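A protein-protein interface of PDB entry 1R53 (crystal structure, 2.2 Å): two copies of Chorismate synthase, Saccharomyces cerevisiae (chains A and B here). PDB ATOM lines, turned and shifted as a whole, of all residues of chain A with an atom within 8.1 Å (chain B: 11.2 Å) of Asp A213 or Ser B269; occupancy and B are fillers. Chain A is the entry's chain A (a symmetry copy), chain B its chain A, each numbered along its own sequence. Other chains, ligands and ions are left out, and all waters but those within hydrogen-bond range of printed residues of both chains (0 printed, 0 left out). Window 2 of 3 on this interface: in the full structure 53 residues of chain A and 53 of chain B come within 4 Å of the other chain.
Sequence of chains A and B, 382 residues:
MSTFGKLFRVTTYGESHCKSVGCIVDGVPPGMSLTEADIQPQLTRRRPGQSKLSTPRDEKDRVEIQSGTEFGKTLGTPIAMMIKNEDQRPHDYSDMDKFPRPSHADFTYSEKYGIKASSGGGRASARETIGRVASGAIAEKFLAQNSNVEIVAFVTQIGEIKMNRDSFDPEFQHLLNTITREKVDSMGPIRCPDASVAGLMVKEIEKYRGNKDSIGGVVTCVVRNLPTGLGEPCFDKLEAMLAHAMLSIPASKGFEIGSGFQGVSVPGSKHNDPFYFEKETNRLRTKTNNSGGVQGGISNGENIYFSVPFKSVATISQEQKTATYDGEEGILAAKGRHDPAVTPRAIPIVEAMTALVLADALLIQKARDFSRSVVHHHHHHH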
ATOM      1  N   GLU A 204     -18.517  25.870  26.422  1.00  0.00           N
ATOM      2  CA  GLU A 204     -18.657  24.431  26.665  1.00  0.00           C
ATOM      3  C   GLU A 204     -17.490  23.724  25.977  1.00  0.00           C
ATOM      4  O   GLU A 204     -16.818  22.865  26.557  1.00  0.00           O
ATOM      5  CB  GLU A 204     -20.006  23.940  26.124  1.00  0.00           C
ATOM      6  CG  GLU A 204     -20.335  22.474  26.372  1.00  0.00           C
ATOM      7  CD  GLU A 204     -21.008  22.209  27.694  1.00  0.00           C
ATOM      8  OE1 GLU A 204     -20.837  23.034  28.590  1.00  0.00           O
ATOM      9  OE2 GLU A 204     -21.697  21.166  27.837  1.00  0.00           O
ATOM     10  N   ILE A 205     -17.218  24.101  24.735  1.00  0.00           N
ATOM     11  CA  ILE A 205     -16.118  23.473  24.031  1.00  0.00           C
ATOM     12  C   ILE A 205     -14.812  23.697  24.745  1.00  0.00           C
ATOM     13  O   ILE A 205     -13.965  22.824  24.733  1.00  0.00           O
ATOM     14  CB  ILE A 205     -16.027  23.965  22.603  1.00  0.00           C
ATOM     15  CG1 ILE A 205     -17.186  23.348  21.794  1.00  0.00           C
ATOM     16  CG2 ILE A 205     -14.643  23.549  21.960  1.00  0.00           C
ATOM     17  CD1 ILE A 205     -17.268  23.895  20.406  1.00  0.00           C
ATOM     18  N   GLU A 206     -14.643  24.871  25.351  1.00  0.00           N
ATOM     19  CA  GLU A 206     -13.394  25.184  26.016  1.00  0.00           C
ATOM     20  C   GLU A 206     -13.285  24.514  27.378  1.00  0.00           C
ATOM     21  O   GLU A 206     -12.240  24.075  27.734  1.00  0.00           O
ATOM     22  CB  GLU A 206     -13.190  26.684  26.082  1.00  0.00           C
ATOM     23  CG  GLU A 206     -12.862  27.255  24.709  1.00  0.00           C
ATOM     24  CD  GLU A 206     -11.567  26.678  24.124  1.00  0.00           C
ATOM     25  OE1 GLU A 206     -10.516  26.815  24.810  1.00  0.00           O
ATOM     26  OE2 GLU A 206     -11.606  26.092  22.994  1.00  0.00           O
ATOM     27  N   LYS A 207     -14.367  24.410  28.118  1.00  0.00           N
ATOM     28  CA  LYS A 207     -14.412  23.537  29.280  1.00  0.00           C
ATOM     29  C   LYS A 207     -13.866  22.129  28.952  1.00  0.00           C
ATOM     30  O   LYS A 207     -12.914  21.678  29.592  1.00  0.00           O
ATOM     31  CB  LYS A 207     -15.827  23.453  29.801  1.00  0.00           C
ATOM     32  CG  LYS A 207     -16.044  22.415  30.868  1.00  0.00           C
ATOM     33  CD  LYS A 207     -17.322  22.673  31.639  1.00  0.00           C
ATOM     34  CE  LYS A 207     -18.496  21.935  31.091  1.00  0.00           C
ATOM     35  NZ  LYS A 207     -19.457  21.574  32.183  1.00  0.00           N
ATOM     36  N   TYR A 208     -14.389  21.468  27.920  1.00  0.00           N
ATOM     37  CA  TYR A 208     -13.953  20.113  27.619  1.00  0.00           C
ATOM     38  C   TYR A 208     -12.562  20.017  27.015  1.00  0.00           C
ATOM     39  O   TYR A 208     -11.854  19.025  27.247  1.00  0.00           O
ATOM     40  CB  TYR A 208     -15.014  19.383  26.787  1.00  0.00           C
ATOM     41  CG  TYR A 208     -16.193  19.065  27.682  1.00  0.00           C
ATOM     42  CD1 TYR A 208     -16.045  18.247  28.792  1.00  0.00           C
ATOM     43  CD2 TYR A 208     -17.426  19.639  27.458  1.00  0.00           C
ATOM     44  CE1 TYR A 208     -17.105  18.000  29.622  1.00  0.00           C
ATOM     45  CE2 TYR A 208     -18.447  19.413  28.261  1.00  0.00           C
ATOM     46  CZ  TYR A 208     -18.315  18.580  29.318  1.00  0.00           C
ATOM     47  OH  TYR A 208     -19.400  18.391  30.092  1.00  0.00           O
ATOM     48  N   ARG A 209     -12.150  21.045  26.284  1.00  0.00           N
ATOM     49  CA  ARG A 209     -10.814  21.075  25.721  1.00  0.00           C
ATOM     50  C   ARG A 209      -9.770  21.189  26.849  1.00  0.00           C
ATOM     51  O   ARG A 209      -8.703  20.586  26.772  1.00  0.00           O
ATOM     52  CB  ARG A 209     -10.684  22.246  24.743  1.00  0.00           C
ATOM     53  CG  ARG A 209      -9.394  22.244  23.860  1.00  0.00           C
ATOM     54  CD  ARG A 209      -9.429  23.267  22.664  1.00  0.00           C
ATOM     55  NE  ARG A 209     -10.405  22.891  21.607  1.00  0.00           N
ATOM     56  CZ  ARG A 209     -10.427  23.382  20.355  1.00  0.00           C
ATOM     57  NH1 ARG A 209      -9.529  24.284  19.953  1.00  0.00           N
ATOM     58  NH2 ARG A 209     -11.357  22.962  19.488  1.00  0.00           N
ATOM     59  N   GLY A 210     -10.127  21.914  27.912  1.00  0.00           N
ATOM     60  CA  GLY A 210      -9.273  22.114  29.056  1.00  0.00           C
ATOM     61  C   GLY A 210      -9.061  20.799  29.777  1.00  0.00           C
ATOM     62  O   GLY A 210      -7.953  20.504  30.248  1.00  0.00           O
ATOM     63  N   ASN A 211     -10.129  20.003  29.850  1.00  0.00           N
ATOM     64  CA  ASN A 211     -10.104  18.662  30.454  1.00  0.00           C
ATOM     65  C   ASN A 211      -9.547  17.550  29.567  1.00  0.00           C
ATOM     66  O   ASN A 211      -9.666  16.387  29.915  1.00  0.00           O
ATOM     67  CB  ASN A 211     -11.533  18.276  30.841  1.00  0.00           C
ATOM     68  CG  ASN A 211     -12.158  19.228  31.871  1.00  0.00           C
ATOM     69  OD1 ASN A 211     -11.455  19.942  32.557  1.00  0.00           O
ATOM     70  ND2 ASN A 211     -13.503  19.194  32.000  1.00  0.00           N
ATOM     71  N   LYS A 212      -8.987  17.893  28.415  1.00  0.00           N
ATOM     72  CA  LYS A 212      -8.510  16.926  27.412  1.00  0.00           C
ATOM     73  C   LYS A 212      -9.596  15.886  27.074  1.00  0.00           C
ATOM     74  O   LYS A 212      -9.336  14.687  26.911  1.00  0.00           O
ATOM     75  CB  LYS A 212      -7.219  16.271  27.880  1.00  0.00           C
ATOM     76  CG  LYS A 212      -6.078  17.259  28.186  1.00  0.00           C
ATOM     77  CD  LYS A 212      -4.736  16.512  28.346  1.00  0.00           C
ATOM     78  CE  LYS A 212      -3.610  17.419  28.871  1.00  0.00           C
ATOM     79  NZ  LYS A 212      -3.830  17.857  30.319  1.00  0.00           N
ATOM     80  N   ASP A 213     -10.823  16.401  27.035  1.00  0.00           N
ATOM     81  CA  ASP A 213     -12.035  15.657  26.770  1.00  0.00           C
ATOM     82  C   ASP A 213     -12.705  16.205  25.493  1.00  0.00           C
ATOM     83  O   ASP A 213     -12.235  17.164  24.883  1.00  0.00           O
ATOM     84  CB  ASP A 213     -12.970  15.820  27.960  1.00  0.00           C
ATOM     85  CG  ASP A 213     -13.816  14.595  28.228  1.00  0.00           C
ATOM     86  OD1 ASP A 213     -14.067  13.813  27.299  1.00  0.00           O
ATOM     87  OD2 ASP A 213     -14.333  14.369  29.339  1.00  0.00           O
ATOM     88  N   SER A 214     -13.801  15.570  25.080  1.00  0.00           N
ATOM     89  CA  SER A 214     -14.600  16.078  23.977  1.00  0.00           C
ATOM     90  C   SER A 214     -16.075  15.935  24.277  1.00  0.00           C
ATOM     91  O   SER A 214     -16.475  15.273  25.258  1.00  0.00           O
ATOM     92  CB  SER A 214     -14.244  15.309  22.743  1.00  0.00           C
ATOM     93  OG  SER A 214     -14.565  13.937  22.933  1.00  0.00           O
ATOM     94  N   ILE A 215     -16.896  16.614  23.481  1.00  0.00           N
ATOM     95  CA  ILE A 215     -18.339  16.496  23.598  1.00  0.00           C
ATOM     96  C   ILE A 215     -19.043  16.708  22.256  1.00  0.00           C
ATOM     97  O   ILE A 215     -18.528  17.366  21.328  1.00  0.00           O
ATOM     98  CB  ILE A 215     -18.897  17.380  24.749  1.00  0.00           C
ATOM     99  CG1 ILE A 215     -20.276  16.896  25.185  1.00  0.00           C
ATOM    100  CG2 ILE A 215     -18.897  18.847  24.393  1.00  0.00           C
ATOM    101  CD1 ILE A 215     -20.613  17.168  26.576  1.00  0.00           C
ATOM    102  N   SER A 312     -18.752  12.686  20.027  1.00  0.00           N
ATOM    103  CA  SER A 312     -17.381  13.229  20.026  1.00  0.00           C
ATOM    104  C   SER A 312     -16.243  12.225  19.798  1.00  0.00           C
ATOM    105  O   SER A 312     -15.208  12.579  19.239  1.00  0.00           O
ATOM    106  CB  SER A 312     -17.144  13.902  21.370  1.00  0.00           C
ATOM    107  OG  SER A 312     -16.601  15.174  21.167  1.00  0.00           O
ATOM    108  N   VAL A 313     -16.407  10.989  20.245  1.00  0.00           N
ATOM    109  CA  VAL A 313     -15.307   9.993  20.139  1.00  0.00           C
ATOM    110  C   VAL A 313     -15.645   8.778  19.239  1.00  0.00           C
ATOM    111  O   VAL A 313     -16.509   7.951  19.565  1.00  0.00           O
ATOM    112  CB  VAL A 313     -14.828   9.495  21.537  1.00  0.00           C
ATOM    113  CG1 VAL A 313     -13.885  10.499  22.161  1.00  0.00           C
ATOM    114  CG2 VAL A 313     -16.011   9.232  22.461  1.00  0.00           C
ATOM    115  N   ARG A 337     -10.396   8.568  19.683  1.00  0.00           N
ATOM    116  CA  ARG A 337      -9.716   9.860  19.647  1.00  0.00           C
ATOM    117  C   ARG A 337     -10.738  10.984  19.839  1.00  0.00           C
ATOM    118  O   ARG A 337     -11.834  10.920  19.283  1.00  0.00           O
ATOM    119  CB  ARG A 337      -8.961  10.028  18.319  1.00  0.00           C
ATOM    120  N   HIS A 338     -10.372  11.996  20.632  1.00  0.00           N
ATOM    121  CA  HIS A 338     -11.265  13.124  20.969  1.00  0.00           C
ATOM    122  C   HIS A 338     -11.270  14.183  19.860  1.00  0.00           C
ATOM    123  O   HIS A 338     -10.378  14.185  19.002  1.00  0.00           O
ATOM    124  CB  HIS A 338     -10.847  13.781  22.305  1.00  0.00           C
ATOM    125  CG  HIS A 338     -11.171  12.959  23.520  1.00  0.00           C
ATOM    126  ND1 HIS A 338     -10.217  12.242  24.206  1.00  0.00           N
ATOM    127  CD2 HIS A 338     -12.338  12.747  24.175  1.00  0.00           C
ATOM    128  CE1 HIS A 338     -10.783  11.619  25.227  1.00  0.00           C
ATOM    129  NE2 HIS A 338     -12.072  11.907  25.228  1.00  0.00           N
ATOM    130  N   ASP A 339     -12.262  15.082  19.907  1.00  0.00           N
ATOM    131  CA  ASP A 339     -12.430  16.185  18.938  1.00  0.00           C
ATOM    132  C   ASP A 339     -12.081  17.637  19.455  1.00  0.00           C
ATOM    133  O   ASP A 339     -10.954  18.064  19.203  1.00  0.00           O
ATOM    134  CB  ASP A 339     -13.783  16.038  18.246  1.00  0.00           C
ATOM    135  CG  ASP A 339     -13.743  14.963  17.159  1.00  0.00           C
ATOM    136  OD1 ASP A 339     -13.803  15.304  15.941  1.00  0.00           O
ATOM    137  OD2 ASP A 339     -13.611  13.747  17.437  1.00  0.00           O
ATOM    138  N   PRO A 340     -12.939  18.430  20.117  1.00  0.00           N
ATOM    139  CA  PRO A 340     -14.412  18.362  20.151  1.00  0.00           C
ATOM    140  C   PRO A 340     -15.098  19.323  19.159  1.00  0.00           C
ATOM    141  O   PRO A 340     -16.145  19.885  19.463  1.00  0.00           O
ATOM    142  CB  PRO A 340     -14.746  18.802  21.589  1.00  0.00           C
ATOM    143  CG  PRO A 340     -13.413  19.450  22.166  1.00  0.00           C
ATOM    144  CD  PRO A 340     -12.432  19.490  21.011  1.00  0.00           C
ATOM    145  N   ALA A 341     -14.533  19.499  17.973  1.00  0.00           N
ATOM    146  CA  ALA A 341     -15.181  20.314  16.962  1.00  0.00           C
ATOM    147  C   ALA A 341     -15.913  19.433  15.939  1.00  0.00           C
ATOM    148  O   ALA A 341     -16.189  19.883  14.820  1.00  0.00           O
ATOM    149  CB  ALA A 341     -14.155  21.221  16.271  1.00  0.00           C
ATOM    150  N   PHE B 168     -26.481   5.234  29.970  1.00  0.00           N
ATOM    151  CA  PHE B 168     -25.582   5.091  31.125  1.00  0.00           C
ATOM    152  C   PHE B 168     -26.229   4.515  32.366  1.00  0.00           C
ATOM    153  O   PHE B 168     -25.565   4.316  33.353  1.00  0.00           O
ATOM    154  CB  PHE B 168     -24.941   6.461  31.480  1.00  0.00           C
ATOM    155  CG  PHE B 168     -24.164   7.023  30.341  1.00  0.00           C
ATOM    156  CD1 PHE B 168     -22.894   6.560  30.086  1.00  0.00           C
ATOM    157  CD2 PHE B 168     -24.757   7.880  29.436  1.00  0.00           C
ATOM    158  CE1 PHE B 168     -22.184   7.002  29.003  1.00  0.00           C
ATOM    159  CE2 PHE B 168     -24.043   8.340  28.337  1.00  0.00           C
ATOM    160  CZ  PHE B 168     -22.748   7.888  28.118  1.00  0.00           C
ATOM    161  N   SER B 259     -26.565   5.962  22.388  1.00  0.00           N
ATOM    162  CA  SER B 259     -26.627   7.159  23.238  1.00  0.00           C
ATOM    163  C   SER B 259     -27.479   8.237  22.566  1.00  0.00           C
ATOM    164  O   SER B 259     -28.086   9.042  23.248  1.00  0.00           O
ATOM    165  CB  SER B 259     -25.221   7.692  23.584  1.00  0.00           C
ATOM    166  OG  SER B 259     -24.500   8.057  22.392  1.00  0.00           O
ATOM    167  N   GLY B 263     -27.300  11.442  24.605  1.00  0.00           N
ATOM    168  CA  GLY B 263     -25.874  11.380  24.924  1.00  0.00           C
ATOM    169  C   GLY B 263     -24.993  12.534  24.426  1.00  0.00           C
ATOM    170  O   GLY B 263     -23.787  12.580  24.734  1.00  0.00           O
ATOM    171  N   VAL B 264     -25.568  13.428  23.634  1.00  0.00           N
ATOM    172  CA  VAL B 264     -24.924  14.671  23.204  1.00  0.00           C
ATOM    173  C   VAL B 264     -24.497  15.555  24.411  1.00  0.00           C
ATOM    174  O   VAL B 264     -23.501  16.275  24.343  1.00  0.00           O
ATOM    175  CB  VAL B 264     -25.890  15.479  22.254  1.00  0.00           C
ATOM    176  CG1 VAL B 264     -25.359  16.821  21.982  1.00  0.00           C
ATOM    177  CG2 VAL B 264     -26.127  14.727  20.952  1.00  0.00           C
ATOM    178  N   SER B 265     -25.266  15.465  25.494  1.00  0.00           N
ATOM    179  CA  SER B 265     -25.001  16.110  26.750  1.00  0.00           C
ATOM    180  C   SER B 265     -23.883  15.469  27.598  1.00  0.00           C
ATOM    181  O   SER B 265     -23.517  16.034  28.606  1.00  0.00           O
ATOM    182  CB  SER B 265     -26.302  16.103  27.602  1.00  0.00           C
ATOM    183  OG  SER B 265     -27.279  16.980  27.031  1.00  0.00           O
ATOM    184  N   VAL B 266     -23.358  14.307  27.212  1.00  0.00           N
ATOM    185  CA  VAL B 266     -22.368  13.585  28.031  1.00  0.00           C
ATOM    186  C   VAL B 266     -21.001  13.592  27.363  1.00  0.00           C
ATOM    187  O   VAL B 266     -20.911  13.275  26.202  1.00  0.00           O
ATOM    188  CB  VAL B 266     -22.820  12.133  28.298  1.00  0.00           C
ATOM    189  CG1 VAL B 266     -21.801  11.383  29.132  1.00  0.00           C
ATOM    190  CG2 VAL B 266     -24.167  12.134  29.040  1.00  0.00           C
ATOM    191  N   PRO B 267     -19.942  13.984  28.082  1.00  0.00           N
ATOM    192  CA  PRO B 267     -18.591  14.014  27.503  1.00  0.00           C
ATOM    193  C   PRO B 267     -18.128  12.675  26.940  1.00  0.00           C
ATOM    194  O   PRO B 267     -18.591  11.609  27.376  1.00  0.00           O
ATOM    195  CB  PRO B 267     -17.690  14.455  28.684  1.00  0.00           C
ATOM    196  CG  PRO B 267     -18.523  14.505  29.903  1.00  0.00           C
ATOM    197  CD  PRO B 267     -19.959  14.469  29.474  1.00  0.00           C
ATOM    198  N   GLY B 268     -17.209  12.736  25.992  1.00  0.00           N
ATOM    199  CA  GLY B 268     -16.660  11.547  25.359  1.00  0.00           C
ATOM    200  C   GLY B 268     -16.007  10.595  26.339  1.00  0.00           C
ATOM    201  O   GLY B 268     -16.122   9.374  26.216  1.00  0.00           O
ATOM    202  N   SER B 269     -15.316  11.144  27.338  1.00  0.00           N
ATOM    203  CA  SER B 269     -14.666  10.300  28.342  1.00  0.00           C
ATOM    204  C   SER B 269     -15.650   9.278  28.964  1.00  0.00           C
ATOM    205  O   SER B 269     -15.312   8.102  29.093  1.00  0.00           O
ATOM    206  CB  SER B 269     -14.033  11.148  29.463  1.00  0.00           C
ATOM    207  OG  SER B 269     -14.965  12.099  29.975  1.00  0.00           O
ATOM    208  N   LYS B 270     -16.846   9.737  29.352  1.00  0.00           N
ATOM    209  CA  LYS B 270     -17.858   8.854  29.924  1.00  0.00           C
ATOM    210  C   LYS B 270     -18.447   7.838  28.919  1.00  0.00           C
ATOM    211  O   LYS B 270     -18.840   6.750  29.299  1.00  0.00           O
ATOM    212  CB  LYS B 270     -18.997   9.658  30.532  1.00  0.00           C
ATOM    213  CG  LYS B 270     -18.585  10.538  31.675  1.00  0.00           C
ATOM    214  CD  LYS B 270     -19.773  10.826  32.600  1.00  0.00           C
ATOM    215  CE  LYS B 270     -19.346  11.598  33.855  1.00  0.00           C
ATOM    216  NZ  LYS B 270     -20.383  11.389  34.930  1.00  0.00           N
ATOM    217  N   HIS B 271     -18.526   8.191  27.658  1.00  0.00           N
ATOM    218  CA  HIS B 271     -18.938   7.229  26.634  1.00  0.00           C
ATOM    219  C   HIS B 271     -17.922   6.091  26.536  1.00  0.00           C
ATOM    220  O   HIS B 271     -18.306   4.935  26.394  1.00  0.00           O
ATOM    221  CB  HIS B 271     -19.074   7.882  25.255  1.00  0.00           C
ATOM    222  CG  HIS B 271     -20.295   8.738  25.110  1.00  0.00           C
ATOM    223  ND1 HIS B 271     -20.285  10.096  25.338  1.00  0.00           N
ATOM    224  CD2 HIS B 271     -21.554   8.434  24.734  1.00  0.00           C
ATOM    225  CE1 HIS B 271     -21.486  10.592  25.104  1.00  0.00           C
ATOM    226  NE2 HIS B 271     -22.277   9.602  24.748  1.00  0.00           N
ATOM    227  N   ASN B 272     -16.633   6.419  26.627  1.00  0.00           N
ATOM    228  CA  ASN B 272     -15.590   5.457  26.267  1.00  0.00           C
ATOM    229  C   ASN B 272     -14.813   4.812  27.392  1.00  0.00           C
ATOM    230  O   ASN B 272     -14.201   3.784  27.167  1.00  0.00           O
ATOM    231  CB  ASN B 272     -14.615   6.071  25.259  1.00  0.00           C
ATOM    232  CG  ASN B 272     -15.144   5.989  23.837  1.00  0.00           C
ATOM    233  OD1 ASN B 272     -16.288   6.402  23.541  1.00  0.00           O
ATOM    234  ND2 ASN B 272     -14.333   5.419  22.949  1.00  0.00           N
ATOM    235  N   ASP B 273     -14.843   5.370  28.594  1.00  0.00           N
ATOM    236  CA  ASP B 273     -13.965   4.856  29.650  1.00  0.00           C
ATOM    237  C   ASP B 273     -14.444   3.454  30.043  1.00  0.00           C
ATOM    238  O   ASP B 273     -15.639   3.200  30.021  1.00  0.00           O
ATOM    239  CB  ASP B 273     -13.944   5.779  30.883  1.00  0.00           C
ATOM    240  CG  ASP B 273     -13.075   7.043  30.688  1.00  0.00           C
ATOM    241  OD1 ASP B 273     -12.423   7.261  29.642  1.00  0.00           O
ATOM    242  OD2 ASP B 273     -13.009   7.896  31.562  1.00  0.00           O
ATOM    243  N   PRO B 274     -13.514   2.550  30.371  1.00  0.00           N
ATOM    244  CA  PRO B 274     -13.882   1.184  30.804  1.00  0.00           C
ATOM    245  C   PRO B 274     -14.718   1.089  32.108  1.00  0.00           C
ATOM    246  O   PRO B 274     -15.331   0.054  32.332  1.00  0.00           O
ATOM    247  CB  PRO B 274     -12.526   0.463  30.957  1.00  0.00           C
ATOM    248  CG  PRO B 274     -11.454   1.547  30.944  1.00  0.00           C
ATOM    249  CD  PRO B 274     -12.050   2.752  30.289  1.00  0.00           C
ATOM    250  N   PHE B 275     -14.732   2.140  32.936  1.00  0.00           N
ATOM    251  CA  PHE B 275     -15.545   2.193  34.176  1.00  0.00           C
ATOM    252  C   PHE B 275     -16.170   3.596  34.329  1.00  0.00           C
ATOM    253  O   PHE B 275     -15.594   4.584  33.858  1.00  0.00           O
ATOM    254  CB  PHE B 275     -14.689   1.850  35.419  1.00  0.00           C
ATOM    255  CG  PHE B 275     -13.837   0.608  35.254  1.00  0.00           C
ATOM    256  CD1 PHE B 275     -14.322  -0.645  35.631  1.00  0.00           C
ATOM    257  CD2 PHE B 275     -12.561   0.688  34.699  1.00  0.00           C
ATOM    258  CE1 PHE B 275     -13.546  -1.807  35.455  1.00  0.00           C
ATOM    259  CE2 PHE B 275     -11.772  -0.465  34.524  1.00  0.00           C
ATOM    260  CZ  PHE B 275     -12.266  -1.715  34.905  1.00  0.00           C
ATOM    261  N   TYR B 276     -17.339   3.681  34.971  1.00  0.00           N
ATOM    262  CA  TYR B 276     -18.078   4.956  35.085  1.00  0.00           C
ATOM    263  C   TYR B 276     -18.698   5.139  36.464  1.00  0.00           C
ATOM    264  O   TYR B 276     -19.377   4.240  36.939  1.00  0.00           O
ATOM    265  CB  TYR B 276     -19.182   5.055  34.003  1.00  0.00           C
ATOM    266  N   ARG B 285     -17.819  -1.021  38.345  1.00  0.00           N
ATOM    267  CA  ARG B 285     -18.887  -0.470  37.489  1.00  0.00           C
ATOM    268  C   ARG B 285     -18.496  -0.438  35.983  1.00  0.00           C
ATOM    269  O   ARG B 285     -18.115   0.611  35.447  1.00  0.00           O
ATOM    270  CB  ARG B 285     -19.296   0.954  38.001  1.00  0.00           C
ATOM    271  N   THR B 286     -18.606  -1.583  35.306  1.00  0.00           N
ATOM    272  CA  THR B 286     -18.146  -1.714  33.907  1.00  0.00           C
ATOM    273  C   THR B 286     -18.890  -0.774  32.904  1.00  0.00           C
ATOM    274  O   THR B 286     -20.050  -0.430  33.101  1.00  0.00           O
ATOM    275  CB  THR B 286     -18.169  -3.226  33.464  1.00  0.00           C
ATOM    276  OG1 THR B 286     -16.962  -3.873  33.910  1.00  0.00           O
ATOM    277  CG2 THR B 286     -18.098  -3.418  31.934  1.00  0.00           C
ATOM    278  N   LYS B 287     -18.178  -0.342  31.860  1.00  0.00           N
ATOM    279  CA  LYS B 287     -18.736   0.504  30.789  1.00  0.00           C
ATOM    280  C   LYS B 287     -20.064  -0.079  30.273  1.00  0.00           C
ATOM    281  O   LYS B 287     -20.182  -1.293  30.136  1.00  0.00           O
ATOM    282  CB  LYS B 287     -17.701   0.641  29.596  1.00  0.00           C
ATOM    283  N   THR B 288     -21.058   0.786  30.050  1.00  0.00           N
ATOM    284  CA  THR B 288     -22.312   0.411  29.363  1.00  0.00           C
ATOM    285  C   THR B 288     -22.161   0.386  27.828  1.00  0.00           C
ATOM    286  O   THR B 288     -21.184   0.884  27.244  1.00  0.00           O
ATOM    287  CB  THR B 288     -23.518   1.363  29.747  1.00  0.00           C
ATOM    288  OG1 THR B 288     -23.188   2.755  29.557  1.00  0.00           O
ATOM    289  CG2 THR B 288     -23.876   1.249  31.233  1.00  0.00           C
ATOM    290  N   ASN B 290     -23.054   2.156  25.060  1.00  0.00           N
ATOM    291  CA  ASN B 290     -23.392   3.486  24.580  1.00  0.00           C
ATOM    292  C   ASN B 290     -23.440   3.635  23.059  1.00  0.00           C
ATOM    293  O   ASN B 290     -24.055   4.579  22.530  1.00  0.00           O
ATOM    294  CB  ASN B 290     -22.389   4.469  25.168  1.00  0.00           C
ATOM    295  CG  ASN B 290     -22.371   4.406  26.668  1.00  0.00           C
ATOM    296  OD1 ASN B 290     -23.389   4.728  27.316  1.00  0.00           O
ATOM    297  ND2 ASN B 290     -21.227   3.958  27.252  1.00  0.00           N
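Of the 21 printed residues of chain B, 7 touch a printed residue of chain A.
Along chain B the printed residues that touch a printed residue of chain A span positions 264 to 272.
Of the 19 printed residues of chain A, 6 touch a printed residue of chain B.
Among the printed residues, 13 pairs touch across the chains.
The backbone NH of Ile A215 sits at hydrogen-bond distance from the side-chain hydroxyl of Ser A312 (2.7 Å).
The backbone NH of Asp A213 sits at hydrogen-bond distance from the backbone carbonyl oxygen of Tyr A208 (2.8 Å).
OD1 of Asp A213 lies within hydrogen-bond range of NE2 of His A338 (3.4 Å).
ND1 of His B271 sits close to O of Val B266 (3.4 Å).
The backbone carbonyl oxygen (O) of Pro B267 is in hydrogen-bond range of a ring nitrogen (ND1) of His B271, 3.1 Å away.
The side-chain hydroxyl (OG) of Ser A214 sits close to the side-chain hydroxyl (OG) of Ser A312, 3.0 Å away.
Tyr A208 touches just one residue of chain B: Pro B267 (3.7 Å).
No residue of chain B comes within 4 Å of Gly A210.
No residue of chain B comes within 4 Å of Asn A211.
Asp A213 touches just these residues of chain B: Pro B267, Gly B268 and Ser B269.
Of the printed residues of chain B, Ser A214 touches Pro B267 (3.3 Å) and Gly B268 (2.7 Å).
Of the printed residues of chain B, Ile A215 touches Val B264 (3.4 Å), Ser B265 (3.7 Å), Val B266 (3.7 Å) and Pro B267 (3.6 Å).
Of the printed residues of chain B, Val A313 touches Gly B268 and Asn B272.
Of the printed residues of chain A, Val B264 touches Ile A215 (3.4 Å).
Printed residues of chain A within 4 Å of Ser B265: Ile A215 (3.7 Å).
Printed residues of chain A within 4 Å of Pro B267: Tyr A208 (3.7 Å), Asp A213 (3.4 Å), Ser A214 (3.3 Å) and Ile A215 (3.6 Å).
Ser B269 touches just these residues of chain A: Asp A213 and His A338.
His B271 touches none of the printed residues of chain A.
The nearest residue of chain B that does not touch Asp A213 is Lys B270 (5.3 Å).
The nearest residue of chain A that does not touch Ser B269 is Ser A214 (4.8 Å).
The nearest printed residue of chain A that does not touch Asn B272 is Arg A337 (6.0 Å).
Among the printed residues, pairs that only touch across the chains: Val A313 with Asn B272, Ser A214 with Pro B267, Ile A215 with Val B264, Asp A213 with Pro B267, Asp A213 with Gly B268, Ile A215 with Pro B267, Ile A215 with Val B266, Tyr A208 with Pro B267, Ile A215 with Ser B265, Val A313 with Gly B268 and His A338 with Ser B269.
N of Gly B268 sits at hydrogen-bond distance from O of Ser A214.
The side-chain hydroxyl (OG) of Ser B269 sits at hydrogen-bond distance from the side-chain carboxylate (OD2) of Asp A213, at 2.4 Å.
No position is printed for both chains.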
